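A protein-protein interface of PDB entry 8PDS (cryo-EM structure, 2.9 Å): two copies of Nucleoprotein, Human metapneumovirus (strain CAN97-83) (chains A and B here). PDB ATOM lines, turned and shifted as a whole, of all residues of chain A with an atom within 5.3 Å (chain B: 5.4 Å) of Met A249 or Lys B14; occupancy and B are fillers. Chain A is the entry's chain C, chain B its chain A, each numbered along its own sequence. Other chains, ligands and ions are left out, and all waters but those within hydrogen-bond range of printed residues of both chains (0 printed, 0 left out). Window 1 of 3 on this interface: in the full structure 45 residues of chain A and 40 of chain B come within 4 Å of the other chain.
Among the printed residues, pairs that only touch across the chains: Met A249 with Lys B14, Met A249 with Leu B18, Tyr A252 with Tyr B13 and Tyr A252 with Lys B14.
Printed residues of chain A within 4 Å of Lys B14: Met A249 and Tyr A252. Of the printed residues of chain B, Tyr A252 touches Tyr B13 (3.1 Å) and Lys B14 (3.98 Å). Of the printed residues of chain A, Tyr B13 touches Tyr A252 (3.1 Å). Of the printed residues of chain A, Leu B18 touches Met A249 (3.5 Å). The nearest printed residue of chain B that does not touch Met A249 is Leu B312 (4.3 Å).
Of the 10 printed residues of chain A, 2 touch a printed residue of chain B. Hydrophobic or aromatic side chains of chain A that line the printed part of chain B: Met A249 and Tyr A252. Printed residues of chain B that touch a printed residue of chain A: Tyr B13, Lys B14 and Leu B18. Hydrophobic or aromatic side chains of chain B that line the printed part of chain A: Tyr B13 and Leu B18. Along chain B the printed residues that touch a printed residue of chain A span positions 13 to 18.
No position is printed for both chains. Of the 4 pairs that touch across the chains among the printed residues, none has its exchanged pair printed and touching as well.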
ATOM      1  N   PHE A 244     -21.665  -4.337  -9.954  1.00  0.00           N
ATOM      2  CA  PHE A 244     -22.210  -3.008 -10.200  1.00  0.00           C
ATOM      3  C   PHE A 244     -22.444  -2.271  -8.892  1.00  0.00           C
ATOM      4  O   PHE A 244     -22.081  -1.099  -8.754  1.00  0.00           O
ATOM      5  CB  PHE A 244     -23.511  -3.106 -10.998  1.00  0.00           C
ATOM      6  CG  PHE A 244     -24.112  -1.772 -11.343  1.00  0.00           C
ATOM      7  CD1 PHE A 244     -24.914  -1.096 -10.437  1.00  0.00           C
ATOM      8  CD2 PHE A 244     -23.875  -1.192 -12.571  1.00  0.00           C
ATOM      9  CE1 PHE A 244     -25.458   0.124 -10.749  1.00  0.00           C
ATOM     10  CE2 PHE A 244     -24.419   0.030 -12.884  1.00  0.00           C
ATOM     11  CZ  PHE A 244     -25.210   0.687 -11.973  1.00  0.00           C
ATOM     12  N   VAL A 245     -23.049  -2.945  -7.915  1.00  0.00           N
ATOM     13  CA  VAL A 245     -23.303  -2.293  -6.635  1.00  0.00           C
ATOM     14  C   VAL A 245     -21.998  -1.974  -5.915  1.00  0.00           C
ATOM     15  O   VAL A 245     -21.899  -0.954  -5.226  1.00  0.00           O
ATOM     16  CB  VAL A 245     -24.244  -3.151  -5.775  1.00  0.00           C
ATOM     17  CG1 VAL A 245     -24.491  -2.490  -4.433  1.00  0.00           C
ATOM     18  CG2 VAL A 245     -25.551  -3.336  -6.499  1.00  0.00           C
ATOM     19  N   ASN A 246     -20.979  -2.818  -6.063  1.00  0.00           N
ATOM     20  CA  ASN A 246     -19.696  -2.540  -5.427  1.00  0.00           C
ATOM     21  C   ASN A 246     -19.059  -1.274  -5.989  1.00  0.00           C
ATOM     22  O   ASN A 246     -18.599  -0.409  -5.234  1.00  0.00           O
ATOM     23  CB  ASN A 246     -18.766  -3.739  -5.594  1.00  0.00           C
ATOM     24  CG  ASN A 246     -19.065  -4.839  -4.604  1.00  0.00           C
ATOM     25  OD1 ASN A 246     -19.649  -4.595  -3.553  1.00  0.00           O
ATOM     26  ND2 ASN A 246     -18.679  -6.061  -4.940  1.00  0.00           N
ATOM     27  N   ILE A 247     -19.044  -1.135  -7.316  1.00  0.00           N
ATOM     28  CA  ILE A 247     -18.507   0.090  -7.912  1.00  0.00           C
ATOM     29  C   ILE A 247     -19.379   1.290  -7.549  1.00  0.00           C
ATOM     30  O   ILE A 247     -18.877   2.399  -7.321  1.00  0.00           O
ATOM     31  CB  ILE A 247     -18.359  -0.065  -9.435  1.00  0.00           C
ATOM     32  CG1 ILE A 247     -17.713  -1.400  -9.788  1.00  0.00           C
ATOM     33  CG2 ILE A 247     -17.506   1.042  -9.999  1.00  0.00           C
ATOM     34  CD1 ILE A 247     -17.778  -1.724 -11.262  1.00  0.00           C
ATOM     35  N   PHE A 248     -20.695   1.086  -7.479  1.00  0.00           N
ATOM     36  CA  PHE A 248     -21.611   2.178  -7.172  1.00  0.00           C
ATOM     37  C   PHE A 248     -21.389   2.704  -5.755  1.00  0.00           C
ATOM     38  O   PHE A 248     -21.458   3.914  -5.518  1.00  0.00           O
ATOM     39  CB  PHE A 248     -23.047   1.695  -7.392  1.00  0.00           C
ATOM     40  CG  PHE A 248     -24.099   2.709  -7.064  1.00  0.00           C
ATOM     41  CD1 PHE A 248     -24.343   3.769  -7.918  1.00  0.00           C
ATOM     42  CD2 PHE A 248     -24.876   2.578  -5.934  1.00  0.00           C
ATOM     43  CE1 PHE A 248     -25.317   4.696  -7.623  1.00  0.00           C
ATOM     44  CE2 PHE A 248     -25.852   3.500  -5.635  1.00  0.00           C
ATOM     45  CZ  PHE A 248     -26.074   4.559  -6.479  1.00  0.00           C
ATOM     46  N   MET A 249     -21.125   1.810  -4.797  1.00  0.00           N
ATOM     47  CA  MET A 249     -20.686   2.250  -3.472  1.00  0.00           C
ATOM     48  C   MET A 249     -19.304   2.879  -3.498  1.00  0.00           C
ATOM     49  O   MET A 249     -19.040   3.804  -2.724  1.00  0.00           O
ATOM     50  CB  MET A 249     -20.701   1.096  -2.472  1.00  0.00           C
ATOM     51  CG  MET A 249     -21.996   0.356  -2.390  1.00  0.00           C
ATOM     52  SD  MET A 249     -23.223   1.486  -1.722  1.00  0.00           S
ATOM     53  CE  MET A 249     -24.508   1.315  -2.931  1.00  0.00           C
ATOM     54  N   GLN A 250     -18.403   2.387  -4.346  1.00  0.00           N
ATOM     55  CA  GLN A 250     -17.106   3.039  -4.463  1.00  0.00           C
ATOM     56  C   GLN A 250     -17.238   4.461  -4.980  1.00  0.00           C
ATOM     57  O   GLN A 250     -16.324   5.269  -4.788  1.00  0.00           O
ATOM     58  CB  GLN A 250     -16.185   2.232  -5.372  1.00  0.00           C
ATOM     59  CG  GLN A 250     -15.522   1.073  -4.667  1.00  0.00           C
ATOM     60  CD  GLN A 250     -14.599   0.299  -5.568  1.00  0.00           C
ATOM     61  OE1 GLN A 250     -14.504   0.574  -6.760  1.00  0.00           O
ATOM     62  NE2 GLN A 250     -13.901  -0.672  -5.001  1.00  0.00           N
ATOM     63  N   ALA A 251     -18.352   4.785  -5.628  1.00  0.00           N
ATOM     64  CA  ALA A 251     -18.600   6.140  -6.099  1.00  0.00           C
ATOM     65  C   ALA A 251     -19.161   7.062  -5.026  1.00  0.00           C
ATOM     66  O   ALA A 251     -19.372   8.242  -5.310  1.00  0.00           O
ATOM     67  CB  ALA A 251     -19.564   6.115  -7.284  1.00  0.00           C
ATOM     68  N   TYR A 252     -19.387   6.571  -3.807  1.00  0.00           N
ATOM     69  CA  TYR A 252     -20.232   7.280  -2.853  1.00  0.00           C
ATOM     70  C   TYR A 252     -19.733   8.672  -2.490  1.00  0.00           C
ATOM     71  O   TYR A 252     -20.352   9.663  -2.875  1.00  0.00           O
ATOM     72  CB  TYR A 252     -20.393   6.463  -1.571  1.00  0.00           C
ATOM     73  CG  TYR A 252     -21.321   7.118  -0.577  1.00  0.00           C
ATOM     74  CD1 TYR A 252     -22.682   7.198  -0.823  1.00  0.00           C
ATOM     75  CD2 TYR A 252     -20.834   7.676   0.596  1.00  0.00           C
ATOM     76  CE1 TYR A 252     -23.528   7.803   0.073  1.00  0.00           C
ATOM     77  CE2 TYR A 252     -21.676   8.282   1.496  1.00  0.00           C
ATOM     78  CZ  TYR A 252     -23.021   8.343   1.230  1.00  0.00           C
ATOM     79  OH  TYR A 252     -23.868   8.949   2.121  1.00  0.00           O
ATOM     80  N   GLY A 253     -18.613   8.779  -1.788  1.00  0.00           N
ATOM     81  CA  GLY A 253     -18.209  10.079  -1.286  1.00  0.00           C
ATOM     82  C   GLY A 253     -17.499  10.941  -2.307  1.00  0.00           C
ATOM     83  O   GLY A 253     -16.645  11.757  -1.952  1.00  0.00           O
ATOM     84  N   ASP B  10     -19.868   6.797   7.087  1.00  0.00           N
ATOM     85  CA  ASP B  10     -20.163   6.586   5.673  1.00  0.00           C
ATOM     86  C   ASP B  10     -20.844   5.250   5.409  1.00  0.00           C
ATOM     87  O   ASP B  10     -21.704   5.161   4.529  1.00  0.00           O
ATOM     88  CB  ASP B  10     -18.885   6.685   4.843  1.00  0.00           C
ATOM     89  CG  ASP B  10     -18.345   8.091   4.772  1.00  0.00           C
ATOM     90  OD1 ASP B  10     -19.147   9.043   4.848  1.00  0.00           O
ATOM     91  OD2 ASP B  10     -17.116   8.246   4.630  1.00  0.00           O
ATOM     92  N   LEU B  11     -20.461   4.195   6.132  1.00  0.00           N
ATOM     93  CA  LEU B  11     -21.017   2.872   5.856  1.00  0.00           C
ATOM     94  C   LEU B  11     -22.482   2.788   6.262  1.00  0.00           C
ATOM     95  O   LEU B  11     -23.294   2.164   5.566  1.00  0.00           O
ATOM     96  CB  LEU B  11     -20.199   1.803   6.573  1.00  0.00           C
ATOM     97  CG  LEU B  11     -20.471   0.364   6.154  1.00  0.00           C
ATOM     98  CD1 LEU B  11     -19.900   0.107   4.776  1.00  0.00           C
ATOM     99  CD2 LEU B  11     -19.878  -0.586   7.166  1.00  0.00           C
ATOM    100  N   SER B  12     -22.838   3.407   7.389  1.00  0.00           N
ATOM    101  CA  SER B  12     -24.240   3.509   7.766  1.00  0.00           C
ATOM    102  C   SER B  12     -25.031   4.258   6.704  1.00  0.00           C
ATOM    103  O   SER B  12     -26.169   3.896   6.393  1.00  0.00           O
ATOM    104  CB  SER B  12     -24.363   4.204   9.120  1.00  0.00           C
ATOM    105  OG  SER B  12     -25.696   4.170   9.594  1.00  0.00           O
ATOM    106  N   TYR B  13     -24.431   5.298   6.123  1.00  0.00           N
ATOM    107  CA  TYR B  13     -25.100   6.059   5.074  1.00  0.00           C
ATOM    108  C   TYR B  13     -25.271   5.231   3.806  1.00  0.00           C
ATOM    109  O   TYR B  13     -26.304   5.322   3.135  1.00  0.00           O
ATOM    110  CB  TYR B  13     -24.313   7.333   4.784  1.00  0.00           C
ATOM    111  CG  TYR B  13     -24.433   8.374   5.867  1.00  0.00           C
ATOM    112  CD1 TYR B  13     -25.372   8.242   6.876  1.00  0.00           C
ATOM    113  CD2 TYR B  13     -23.611   9.488   5.881  1.00  0.00           C
ATOM    114  CE1 TYR B  13     -25.491   9.185   7.865  1.00  0.00           C
ATOM    115  CE2 TYR B  13     -23.724  10.438   6.868  1.00  0.00           C
ATOM    116  CZ  TYR B  13     -24.665  10.280   7.858  1.00  0.00           C
ATOM    117  OH  TYR B  13     -24.787  11.218   8.851  1.00  0.00           O
ATOM    118  N   LYS B  14     -24.268   4.426   3.457  1.00  0.00           N
ATOM    119  CA  LYS B  14     -24.384   3.553   2.292  1.00  0.00           C
ATOM    120  C   LYS B  14     -25.475   2.509   2.492  1.00  0.00           C
ATOM    121  O   LYS B  14     -26.252   2.219   1.571  1.00  0.00           O
ATOM    122  CB  LYS B  14     -23.045   2.877   2.014  1.00  0.00           C
ATOM    123  CG  LYS B  14     -21.955   3.812   1.540  1.00  0.00           C
ATOM    124  CD  LYS B  14     -20.696   3.039   1.213  1.00  0.00           C
ATOM    125  CE  LYS B  14     -19.464   3.810   1.625  1.00  0.00           C
ATOM    126  NZ  LYS B  14     -18.307   2.909   1.853  1.00  0.00           N
ATOM    127  N   HIS B  15     -25.549   1.927   3.690  1.00  0.00           N
ATOM    128  CA  HIS B  15     -26.618   0.974   3.954  1.00  0.00           C
ATOM    129  C   HIS B  15     -27.981   1.649   3.974  1.00  0.00           C
ATOM    130  O   HIS B  15     -28.971   1.040   3.565  1.00  0.00           O
ATOM    131  CB  HIS B  15     -26.387   0.236   5.268  1.00  0.00           C
ATOM    132  CG  HIS B  15     -27.368  -0.869   5.505  1.00  0.00           C
ATOM    133  ND1 HIS B  15     -28.029  -1.038   6.702  1.00  0.00           N
ATOM    134  CD2 HIS B  15     -27.813  -1.853   4.688  1.00  0.00           C
ATOM    135  CE1 HIS B  15     -28.833  -2.082   6.614  1.00  0.00           C
ATOM    136  NE2 HIS B  15     -28.721  -2.594   5.403  1.00  0.00           N
ATOM    137  N   ALA B  16     -28.060   2.890   4.457  1.00  0.00           N
ATOM    138  CA  ALA B  16     -29.320   3.621   4.396  1.00  0.00           C
ATOM    139  C   ALA B  16     -29.726   3.884   2.953  1.00  0.00           C
ATOM    140  O   ALA B  16     -30.912   3.822   2.612  1.00  0.00           O
ATOM    141  CB  ALA B  16     -29.202   4.932   5.170  1.00  0.00           C
ATOM    142  N   ILE B  17     -28.751   4.189   2.097  1.00  0.00           N
ATOM    143  CA  ILE B  17     -29.022   4.392   0.677  1.00  0.00           C
ATOM    144  C   ILE B  17     -29.581   3.120   0.054  1.00  0.00           C
ATOM    145  O   ILE B  17     -30.593   3.146  -0.656  1.00  0.00           O
ATOM    146  CB  ILE B  17     -27.744   4.858  -0.043  1.00  0.00           C
ATOM    147  CG1 ILE B  17     -27.480   6.332   0.250  1.00  0.00           C
ATOM    148  CG2 ILE B  17     -27.836   4.618  -1.539  1.00  0.00           C
ATOM    149  CD1 ILE B  17     -28.599   7.230  -0.176  1.00  0.00           C
ATOM    150  N   LEU B  18     -28.930   1.984   0.311  1.00  0.00           N
ATOM    151  CA  LEU B  18     -29.365   0.732  -0.303  1.00  0.00           C
ATOM    152  C   LEU B  18     -30.710   0.272   0.246  1.00  0.00           C
ATOM    153  O   LEU B  18     -31.618  -0.074  -0.517  1.00  0.00           O
ATOM    154  CB  LEU B  18     -28.305  -0.346  -0.097  1.00  0.00           C
ATOM    155  CG  LEU B  18     -27.122  -0.232  -1.048  1.00  0.00           C
ATOM    156  CD1 LEU B  18     -26.240  -1.463  -0.979  1.00  0.00           C
ATOM    157  CD2 LEU B  18     -27.656  -0.029  -2.454  1.00  0.00           C
ATOM    158  N   LYS B  19     -30.854   0.265   1.570  1.00  0.00           N
ATOM    159  CA  LYS B  19     -32.050  -0.282   2.202  1.00  0.00           C
ATOM    160  C   LYS B  19     -33.293   0.521   1.840  1.00  0.00           C
ATOM    161  O   LYS B  19     -34.336  -0.049   1.500  1.00  0.00           O
ATOM    162  CB  LYS B  19     -31.846  -0.320   3.716  1.00  0.00           C
ATOM    163  CG  LYS B  19     -33.036  -0.809   4.510  1.00  0.00           C
ATOM    164  CD  LYS B  19     -32.678  -0.918   5.979  1.00  0.00           C
ATOM    165  CE  LYS B  19     -32.487   0.454   6.600  1.00  0.00           C
ATOM    166  NZ  LYS B  19     -32.235   0.367   8.065  1.00  0.00           N
ATOM    167  N   LEU B 312     -20.955  -4.513   1.558  1.00  0.00           N
ATOM    168  CA  LEU B 312     -20.941  -3.576   2.671  1.00  0.00           C
ATOM    169  C   LEU B 312     -20.313  -4.206   3.903  1.00  0.00           C
ATOM    170  O   LEU B 312     -19.692  -3.507   4.711  1.00  0.00           O
ATOM    171  CB  LEU B 312     -22.362  -3.111   2.978  1.00  0.00           C
ATOM    172  CG  LEU B 312     -23.074  -2.242   1.942  1.00  0.00           C
ATOM    173  CD1 LEU B 312     -24.530  -2.062   2.322  1.00  0.00           C
ATOM    174  CD2 LEU B 312     -22.391  -0.896   1.810  1.00  0.00           C
